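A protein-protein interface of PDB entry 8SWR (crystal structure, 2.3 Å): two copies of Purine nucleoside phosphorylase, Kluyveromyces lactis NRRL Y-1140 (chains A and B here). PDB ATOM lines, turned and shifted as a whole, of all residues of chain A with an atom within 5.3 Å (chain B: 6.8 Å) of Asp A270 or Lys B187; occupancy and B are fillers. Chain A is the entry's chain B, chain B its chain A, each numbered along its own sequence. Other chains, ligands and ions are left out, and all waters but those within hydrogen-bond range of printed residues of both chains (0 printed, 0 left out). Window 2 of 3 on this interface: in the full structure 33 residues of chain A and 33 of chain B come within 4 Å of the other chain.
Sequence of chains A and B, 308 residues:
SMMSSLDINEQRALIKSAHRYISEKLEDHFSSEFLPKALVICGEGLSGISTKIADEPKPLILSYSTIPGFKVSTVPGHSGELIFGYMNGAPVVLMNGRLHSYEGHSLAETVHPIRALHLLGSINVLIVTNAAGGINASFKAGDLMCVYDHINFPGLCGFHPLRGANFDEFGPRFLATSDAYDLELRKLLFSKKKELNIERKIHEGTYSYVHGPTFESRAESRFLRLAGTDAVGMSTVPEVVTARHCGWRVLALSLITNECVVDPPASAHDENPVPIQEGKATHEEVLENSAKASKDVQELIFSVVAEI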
ATOM      1  N   ALA A 266       7.995   4.528  35.515  1.00  0.00           N
ATOM      2  CA  ALA A 266       8.450   3.554  34.536  1.00  0.00           C
ATOM      3  C   ALA A 266       7.684   3.712  33.231  1.00  0.00           C
ATOM      4  O   ALA A 266       6.460   3.869  33.222  1.00  0.00           O
ATOM      5  CB  ALA A 266       8.271   2.139  35.080  1.00  0.00           C
ATOM      6  N   SER A 267       8.417   3.684  32.125  1.00  0.00           N
ATOM      7  CA  SER A 267       7.800   3.753  30.814  1.00  0.00           C
ATOM      8  C   SER A 267       7.356   2.368  30.366  1.00  0.00           C
ATOM      9  O   SER A 267       7.979   1.355  30.696  1.00  0.00           O
ATOM     10  CB  SER A 267       8.767   4.349  29.793  1.00  0.00           C
ATOM     11  OG  SER A 267       8.437   3.925  28.484  1.00  0.00           O
ATOM     12  N   ALA A 268       6.259   2.333  29.609  1.00  0.00           N
ATOM     13  CA  ALA A 268       5.769   1.071  29.074  1.00  0.00           C
ATOM     14  C   ALA A 268       6.737   0.446  28.083  1.00  0.00           C
ATOM     15  O   ALA A 268       6.596  -0.740  27.765  1.00  0.00           O
ATOM     16  CB  ALA A 268       4.405   1.271  28.413  1.00  0.00           C
ATOM     17  N   HIS A 269       7.709   1.210  27.587  1.00  0.00           N
ATOM     18  CA  HIS A 269       8.743   0.686  26.709  1.00  0.00           C
ATOM     19  C   HIS A 269       9.969   0.197  27.465  1.00  0.00           C
ATOM     20  O   HIS A 269      10.846  -0.426  26.855  1.00  0.00           O
ATOM     21  CB  HIS A 269       9.160   1.754  25.695  1.00  0.00           C
ATOM     22  CG  HIS A 269       8.007   2.470  25.067  1.00  0.00           C
ATOM     23  ND1 HIS A 269       6.913   1.810  24.551  1.00  0.00           N
ATOM     24  CD2 HIS A 269       7.773   3.791  24.876  1.00  0.00           C
ATOM     25  CE1 HIS A 269       6.057   2.692  24.066  1.00  0.00           C
ATOM     26  NE2 HIS A 269       6.555   3.901  24.250  1.00  0.00           N
ATOM     27  N   ASP A 270      10.054   0.464  28.766  1.00  0.00           N
ATOM     28  CA  ASP A 270      11.160  -0.044  29.563  1.00  0.00           C
ATOM     29  C   ASP A 270      11.037  -1.553  29.725  1.00  0.00           C
ATOM     30  O   ASP A 270       9.980  -2.068  30.099  1.00  0.00           O
ATOM     31  CB  ASP A 270      11.191   0.627  30.935  1.00  0.00           C
ATOM     32  CG  ASP A 270      11.817   2.006  30.898  1.00  0.00           C
ATOM     33  OD1 ASP A 270      11.788   2.696  31.941  1.00  0.00           O
ATOM     34  OD2 ASP A 270      12.339   2.399  29.834  1.00  0.00           O
ATOM     35  N   GLU A 271      12.125  -2.256  29.441  1.00  0.00           N
ATOM     36  CA  GLU A 271      12.206  -3.690  29.660  1.00  0.00           C
ATOM     37  C   GLU A 271      12.752  -4.043  31.036  1.00  0.00           C
ATOM     38  O   GLU A 271      12.541  -5.168  31.505  1.00  0.00           O
ATOM     39  CB  GLU A 271      13.070  -4.310  28.561  1.00  0.00           C
ATOM     40  CG  GLU A 271      12.692  -3.812  27.172  1.00  0.00           C
ATOM     41  CD  GLU A 271      13.638  -4.279  26.088  1.00  0.00           C
ATOM     42  OE1 GLU A 271      13.408  -3.894  24.918  1.00  0.00           O
ATOM     43  OE2 GLU A 271      14.636  -4.970  26.418  1.00  0.00           O
ATOM     44  N   ASN A 272      13.428  -3.105  31.694  1.00  0.00           N
ATOM     45  CA  ASN A 272      13.886  -3.268  33.073  1.00  0.00           C
ATOM     46  C   ASN A 272      13.381  -2.102  33.914  1.00  0.00           C
ATOM     47  O   ASN A 272      14.166  -1.305  34.437  1.00  0.00           O
ATOM     48  CB  ASN A 272      15.409  -3.362  33.126  1.00  0.00           C
ATOM     49  CG  ASN A 272      15.941  -4.563  32.379  1.00  0.00           C
ATOM     50  OD1 ASN A 272      16.130  -4.519  31.162  1.00  0.00           O
ATOM     51  ND2 ASN A 272      16.188  -5.648  33.103  1.00  0.00           N
ATOM     52  N   PRO A 273      12.065  -1.973  34.072  1.00  0.00           N
ATOM     53  CA  PRO A 273      11.521  -0.779  34.722  1.00  0.00           C
ATOM     54  C   PRO A 273      11.623  -0.858  36.235  1.00  0.00           C
ATOM     55  O   PRO A 273      11.505  -1.927  36.836  1.00  0.00           O
ATOM     56  CB  PRO A 273      10.057  -0.781  34.270  1.00  0.00           C
ATOM     57  CG  PRO A 273       9.730  -2.230  34.152  1.00  0.00           C
ATOM     58  CD  PRO A 273      10.999  -2.926  33.707  1.00  0.00           C
ATOM     59  N   CYS B 146      -1.001   8.290  26.383  1.00  0.00           N
ATOM     60  CA  CYS B 146      -1.198   7.427  27.536  1.00  0.00           C
ATOM     61  C   CYS B 146      -0.673   8.132  28.781  1.00  0.00           C
ATOM     62  O   CYS B 146       0.494   8.536  28.830  1.00  0.00           O
ATOM     63  CB  CYS B 146      -0.486   6.095  27.322  1.00  0.00           C
ATOM     64  SG  CYS B 146      -0.553   4.965  28.724  1.00  0.00           S
ATOM     65  N   ASP B 182      -0.936   2.316  36.595  1.00  0.00           N
ATOM     66  CA  ASP B 182      -0.423   0.953  36.526  1.00  0.00           C
ATOM     67  C   ASP B 182       0.457   0.749  35.300  1.00  0.00           C
ATOM     68  O   ASP B 182       0.114   1.172  34.193  1.00  0.00           O
ATOM     69  CB  ASP B 182      -1.604  -0.020  36.508  1.00  0.00           C
ATOM     70  CG  ASP B 182      -1.176  -1.464  36.599  1.00  0.00           C
ATOM     71  OD1 ASP B 182      -0.941  -1.948  37.726  1.00  0.00           O
ATOM     72  OD2 ASP B 182      -1.086  -2.119  35.541  1.00  0.00           O
ATOM     73  N   LEU B 183       1.600   0.092  35.507  1.00  0.00           N
ATOM     74  CA  LEU B 183       2.551  -0.103  34.419  1.00  0.00           C
ATOM     75  C   LEU B 183       2.103  -1.194  33.454  1.00  0.00           C
ATOM     76  O   LEU B 183       2.180  -1.012  32.234  1.00  0.00           O
ATOM     77  CB  LEU B 183       3.936  -0.431  34.975  1.00  0.00           C
ATOM     78  CG  LEU B 183       5.003  -0.581  33.889  1.00  0.00           C
ATOM     79  CD1 LEU B 183       5.170   0.710  33.101  1.00  0.00           C
ATOM     80  CD2 LEU B 183       6.326  -1.025  34.487  1.00  0.00           C
ATOM     81  N   GLU B 184       1.646  -2.336  33.977  1.00  0.00           N
ATOM     82  CA  GLU B 184       1.216  -3.426  33.107  1.00  0.00           C
ATOM     83  C   GLU B 184       0.044  -3.020  32.223  1.00  0.00           C
ATOM     84  O   GLU B 184      -0.046  -3.460  31.072  1.00  0.00           O
ATOM     85  CB  GLU B 184       0.849  -4.652  33.945  1.00  0.00           C
ATOM     86  N   LEU B 185      -0.858  -2.175  32.735  1.00  0.00           N
ATOM     87  CA  LEU B 185      -1.992  -1.733  31.933  1.00  0.00           C
ATOM     88  C   LEU B 185      -1.553  -0.833  30.785  1.00  0.00           C
ATOM     89  O   LEU B 185      -2.182  -0.838  29.722  1.00  0.00           O
ATOM     90  CB  LEU B 185      -3.009  -1.016  32.820  1.00  0.00           C
ATOM     91  CG  LEU B 185      -3.943  -1.929  33.617  1.00  0.00           C
ATOM     92  CD1 LEU B 185      -4.895  -1.116  34.477  1.00  0.00           C
ATOM     93  CD2 LEU B 185      -4.714  -2.855  32.687  1.00  0.00           C
ATOM     94  N   ARG B 186      -0.487  -0.054  30.978  1.00  0.00           N
ATOM     95  CA  ARG B 186       0.029   0.770  29.891  1.00  0.00           C
ATOM     96  C   ARG B 186       0.784  -0.068  28.867  1.00  0.00           C
ATOM     97  O   ARG B 186       0.648   0.155  27.659  1.00  0.00           O
ATOM     98  CB  ARG B 186       0.930   1.876  30.443  1.00  0.00           C
ATOM     99  CG  ARG B 186       0.220   2.831  31.380  1.00  0.00           C
ATOM    100  CD  ARG B 186       1.136   3.961  31.815  1.00  0.00           C
ATOM    101  NE  ARG B 186       1.840   3.661  33.057  1.00  0.00           N
ATOM    102  CZ  ARG B 186       3.160   3.645  33.186  1.00  0.00           C
ATOM    103  NH1 ARG B 186       3.957   3.890  32.159  1.00  0.00           N
ATOM    104  NH2 ARG B 186       3.694   3.378  34.374  1.00  0.00           N
ATOM    105  N   LYS B 187       1.589  -1.027  29.333  1.00  0.00           N
ATOM    106  CA  LYS B 187       2.237  -1.959  28.415  1.00  0.00           C
ATOM    107  C   LYS B 187       1.204  -2.713  27.591  1.00  0.00           C
ATOM    108  O   LYS B 187       1.397  -2.935  26.389  1.00  0.00           O
ATOM    109  CB  LYS B 187       3.116  -2.939  29.191  1.00  0.00           C
ATOM    110  CG  LYS B 187       4.490  -2.406  29.550  1.00  0.00           C
ATOM    111  CD  LYS B 187       5.275  -3.419  30.365  1.00  0.00           C
ATOM    112  CE  LYS B 187       6.771  -3.213  30.203  1.00  0.00           C
ATOM    113  NZ  LYS B 187       7.282  -2.149  31.109  1.00  0.00           N
ATOM    114  N   LEU B 188       0.097  -3.110  28.223  1.00  0.00           N
ATOM    115  CA  LEU B 188      -0.947  -3.835  27.507  1.00  0.00           C
ATOM    116  C   LEU B 188      -1.573  -2.959  26.430  1.00  0.00           C
ATOM    117  O   LEU B 188      -1.898  -3.441  25.340  1.00  0.00           O
ATOM    118  CB  LEU B 188      -2.008  -4.325  28.493  1.00  0.00           C
ATOM    119  CG  LEU B 188      -3.394  -4.712  27.975  1.00  0.00           C
ATOM    120  CD1 LEU B 188      -3.280  -5.842  26.974  1.00  0.00           C
ATOM    121  CD2 LEU B 188      -4.302  -5.111  29.118  1.00  0.00           C
ATOM    122  N   LEU B 189      -1.741  -1.664  26.714  1.00  0.00           N
ATOM    123  CA  LEU B 189      -2.321  -0.761  25.725  1.00  0.00           C
ATOM    124  C   LEU B 189      -1.432  -0.662  24.492  1.00  0.00           C
ATOM    125  O   LEU B 189      -1.914  -0.758  23.357  1.00  0.00           O
ATOM    126  CB  LEU B 189      -2.550   0.622  26.336  1.00  0.00           C
ATOM    127  CG  LEU B 189      -2.835   1.724  25.312  1.00  0.00           C
ATOM    128  CD1 LEU B 189      -4.243   1.580  24.748  1.00  0.00           C
ATOM    129  CD2 LEU B 189      -2.633   3.103  25.919  1.00  0.00           C
ATOM    130  N   PHE B 190      -0.128  -0.470  24.697  1.00  0.00           N
ATOM    131  CA  PHE B 190       0.794  -0.442  23.567  1.00  0.00           C
ATOM    132  C   PHE B 190       0.845  -1.786  22.858  1.00  0.00           C
ATOM    133  O   PHE B 190       1.026  -1.838  21.634  1.00  0.00           O
ATOM    134  CB  PHE B 190       2.188  -0.037  24.039  1.00  0.00           C
ATOM    135  CG  PHE B 190       2.346   1.438  24.261  1.00  0.00           C
ATOM    136  CD1 PHE B 190       2.636   2.282  23.203  1.00  0.00           C
ATOM    137  CD2 PHE B 190       2.207   1.981  25.528  1.00  0.00           C
ATOM    138  CE1 PHE B 190       2.785   3.642  23.405  1.00  0.00           C
ATOM    139  CE2 PHE B 190       2.356   3.338  25.735  1.00  0.00           C
ATOM    140  CZ  PHE B 190       2.645   4.170  24.672  1.00  0.00           C
ATOM    141  N   SER B 191       0.693  -2.882  23.606  1.00  0.00           N
ATOM    142  CA  SER B 191       0.611  -4.198  22.982  1.00  0.00           C
ATOM    143  C   SER B 191      -0.588  -4.288  22.050  1.00  0.00           C
ATOM    144  O   SER B 191      -0.495  -4.856  20.956  1.00  0.00           O
ATOM    145  CB  SER B 191       0.541  -5.284  24.056  1.00  0.00           C
ATOM    146  OG  SER B 191       0.411  -6.570  23.475  1.00  0.00           O
ATOM    147  N   LYS B 192      -1.724  -3.724  22.463  1.00  0.00           N
ATOM    148  CA  LYS B 192      -2.907  -3.743  21.611  1.00  0.00           C
ATOM    149  C   LYS B 192      -2.771  -2.790  20.431  1.00  0.00           C
ATOM    150  O   LYS B 192      -3.326  -3.057  19.361  1.00  0.00           O
ATOM    151  CB  LYS B 192      -4.149  -3.414  22.437  1.00  0.00           C
ATOM    152  CG  LYS B 192      -4.463  -4.473  23.473  1.00  0.00           C
ATOM    153  CD  LYS B 192      -4.452  -5.855  22.838  1.00  0.00           C
ATOM    154  CE  LYS B 192      -3.636  -6.834  23.651  1.00  0.00           C
ATOM    155  NZ  LYS B 192      -3.518  -8.158  22.984  1.00  0.00           N
ATOM    156  N   GLU B 204       3.578   9.077  25.833  1.00  0.00           N
ATOM    157  CA  GLU B 204       3.462   8.831  27.262  1.00  0.00           C
ATOM    158  C   GLU B 204       3.839  10.116  27.976  1.00  0.00           C
ATOM    159  O   GLU B 204       4.895  10.691  27.696  1.00  0.00           O
ATOM    160  CB  GLU B 204       4.366   7.681  27.714  1.00  0.00           C
ATOM    161  CG  GLU B 204       3.632   6.380  27.983  1.00  0.00           C
ATOM    162  CD  GLU B 204       4.486   5.378  28.736  1.00  0.00           C
ATOM    163  OE1 GLU B 204       3.926   4.383  29.242  1.00  0.00           O
ATOM    164  OE2 GLU B 204       5.715   5.586  28.820  1.00  0.00           O
ATOM    165  N   LEU B 251      -6.009   2.922  34.014  1.00  0.00           N
ATOM    166  CA  LEU B 251      -5.462   3.204  32.694  1.00  0.00           C
ATOM    167  C   LEU B 251      -6.169   4.440  32.157  1.00  0.00           C
ATOM    168  O   LEU B 251      -7.397   4.447  32.027  1.00  0.00           O
ATOM    169  CB  LEU B 251      -5.646   2.022  31.742  1.00  0.00           C
ATOM    170  CG  LEU B 251      -5.373   2.329  30.267  1.00  0.00           C
ATOM    171  CD1 LEU B 251      -3.876   2.389  29.997  1.00  0.00           C
ATOM    172  CD2 LEU B 251      -6.047   1.314  29.354  1.00  0.00           C
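No position is printed for both chains. Of the 13 pairs that touch across the chains among the printed residues, none has its exchanged pair printed and touching as well.
Of the 8 printed residues of chain A, 6 touch a printed residue of chain B. Along chain A the printed residues that touch a printed residue of chain B span positions 266 to 273. Of the 14 printed residues of chain B, 5 touch a printed residue of chain A. Hydrophobic or aromatic side chains of chain B that line the printed part of chain A: Leu B183 and Phe B190. Among the printed residues, 13 pairs touch across the chains. Among the printed residues, no Asp or Glu carboxylate lies within 4 Å of a Lys or Arg side-chain nitrogen of the other chain.
Asp A270 touches just one residue of chain B: Lys B187 (2.9 Å). Of chain A, only Ser A267, Ala A268, Asp A270 and Pro A273 come within 4 Å of Lys B187. Printed residues of chain A within 4 Å of Arg B186: Ala A266 and Ala A268. Of the printed residues of chain A, Phe B190 touches Ala A268 (3.7 Å) and His A269 (3.5 Å). Leu B251 touches none of the printed residues of chain A. Ser B191 touches none of the printed residues of chain A. The nearest printed residue of chain A that does not touch Phe B190 is Ser A267 (6.7 Å).
The backbone carbonyl oxygen of Ala A266 sits at hydrogen-bond distance from the guanidinium group of Arg B186, at 2.7 Å. The backbone carbonyl oxygen (O) of Asp A270 is in hydrogen-bond range of the side-chain amino group (NZ) of Lys B187 (2.9 Å). OG of Ser A267 is in hydrogen-bond range of OE2 of Glu B204, 3.2 Å away. The backbone NH of Ala A268 is in hydrogen-bond range of the side-chain carboxylate of Glu B204 (3.1 Å).
Leu B183 touches Ala A266 (CD1 to O, 3.4 Å). O of Ser A267 touches CD1 of Leu B183, 3.8 Å away. Ser A267 touches Lys B187. Ala A268 touches Arg B186. Lys B187 touches Ala A268 (CG to O, 3.2 Å). Phe B190 touches Ala A268. CE1 of His A269 touches CE1 of Phe B190 (3.5 Å). CD2 of Leu B183 touches CG of Pro A273, at 3.6 Å. CG of Pro A273 touches NZ of Lys B187, at 3.9 Å.
The guanidinium group (NE) of Arg B186 sits at hydrogen-bond distance from the backbone carbonyl oxygen (O) of Asp B182. The guanidinium group (NH1) of Arg B186 is in salt-bridge range of the side-chain carboxylate (OE1) of Glu B204, at 3.0 Å. The side-chain hydroxyl (OG) of Ser A267 lies within hydrogen-bond range of the backbone NH (N) of His A269, at 3.0 Å.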
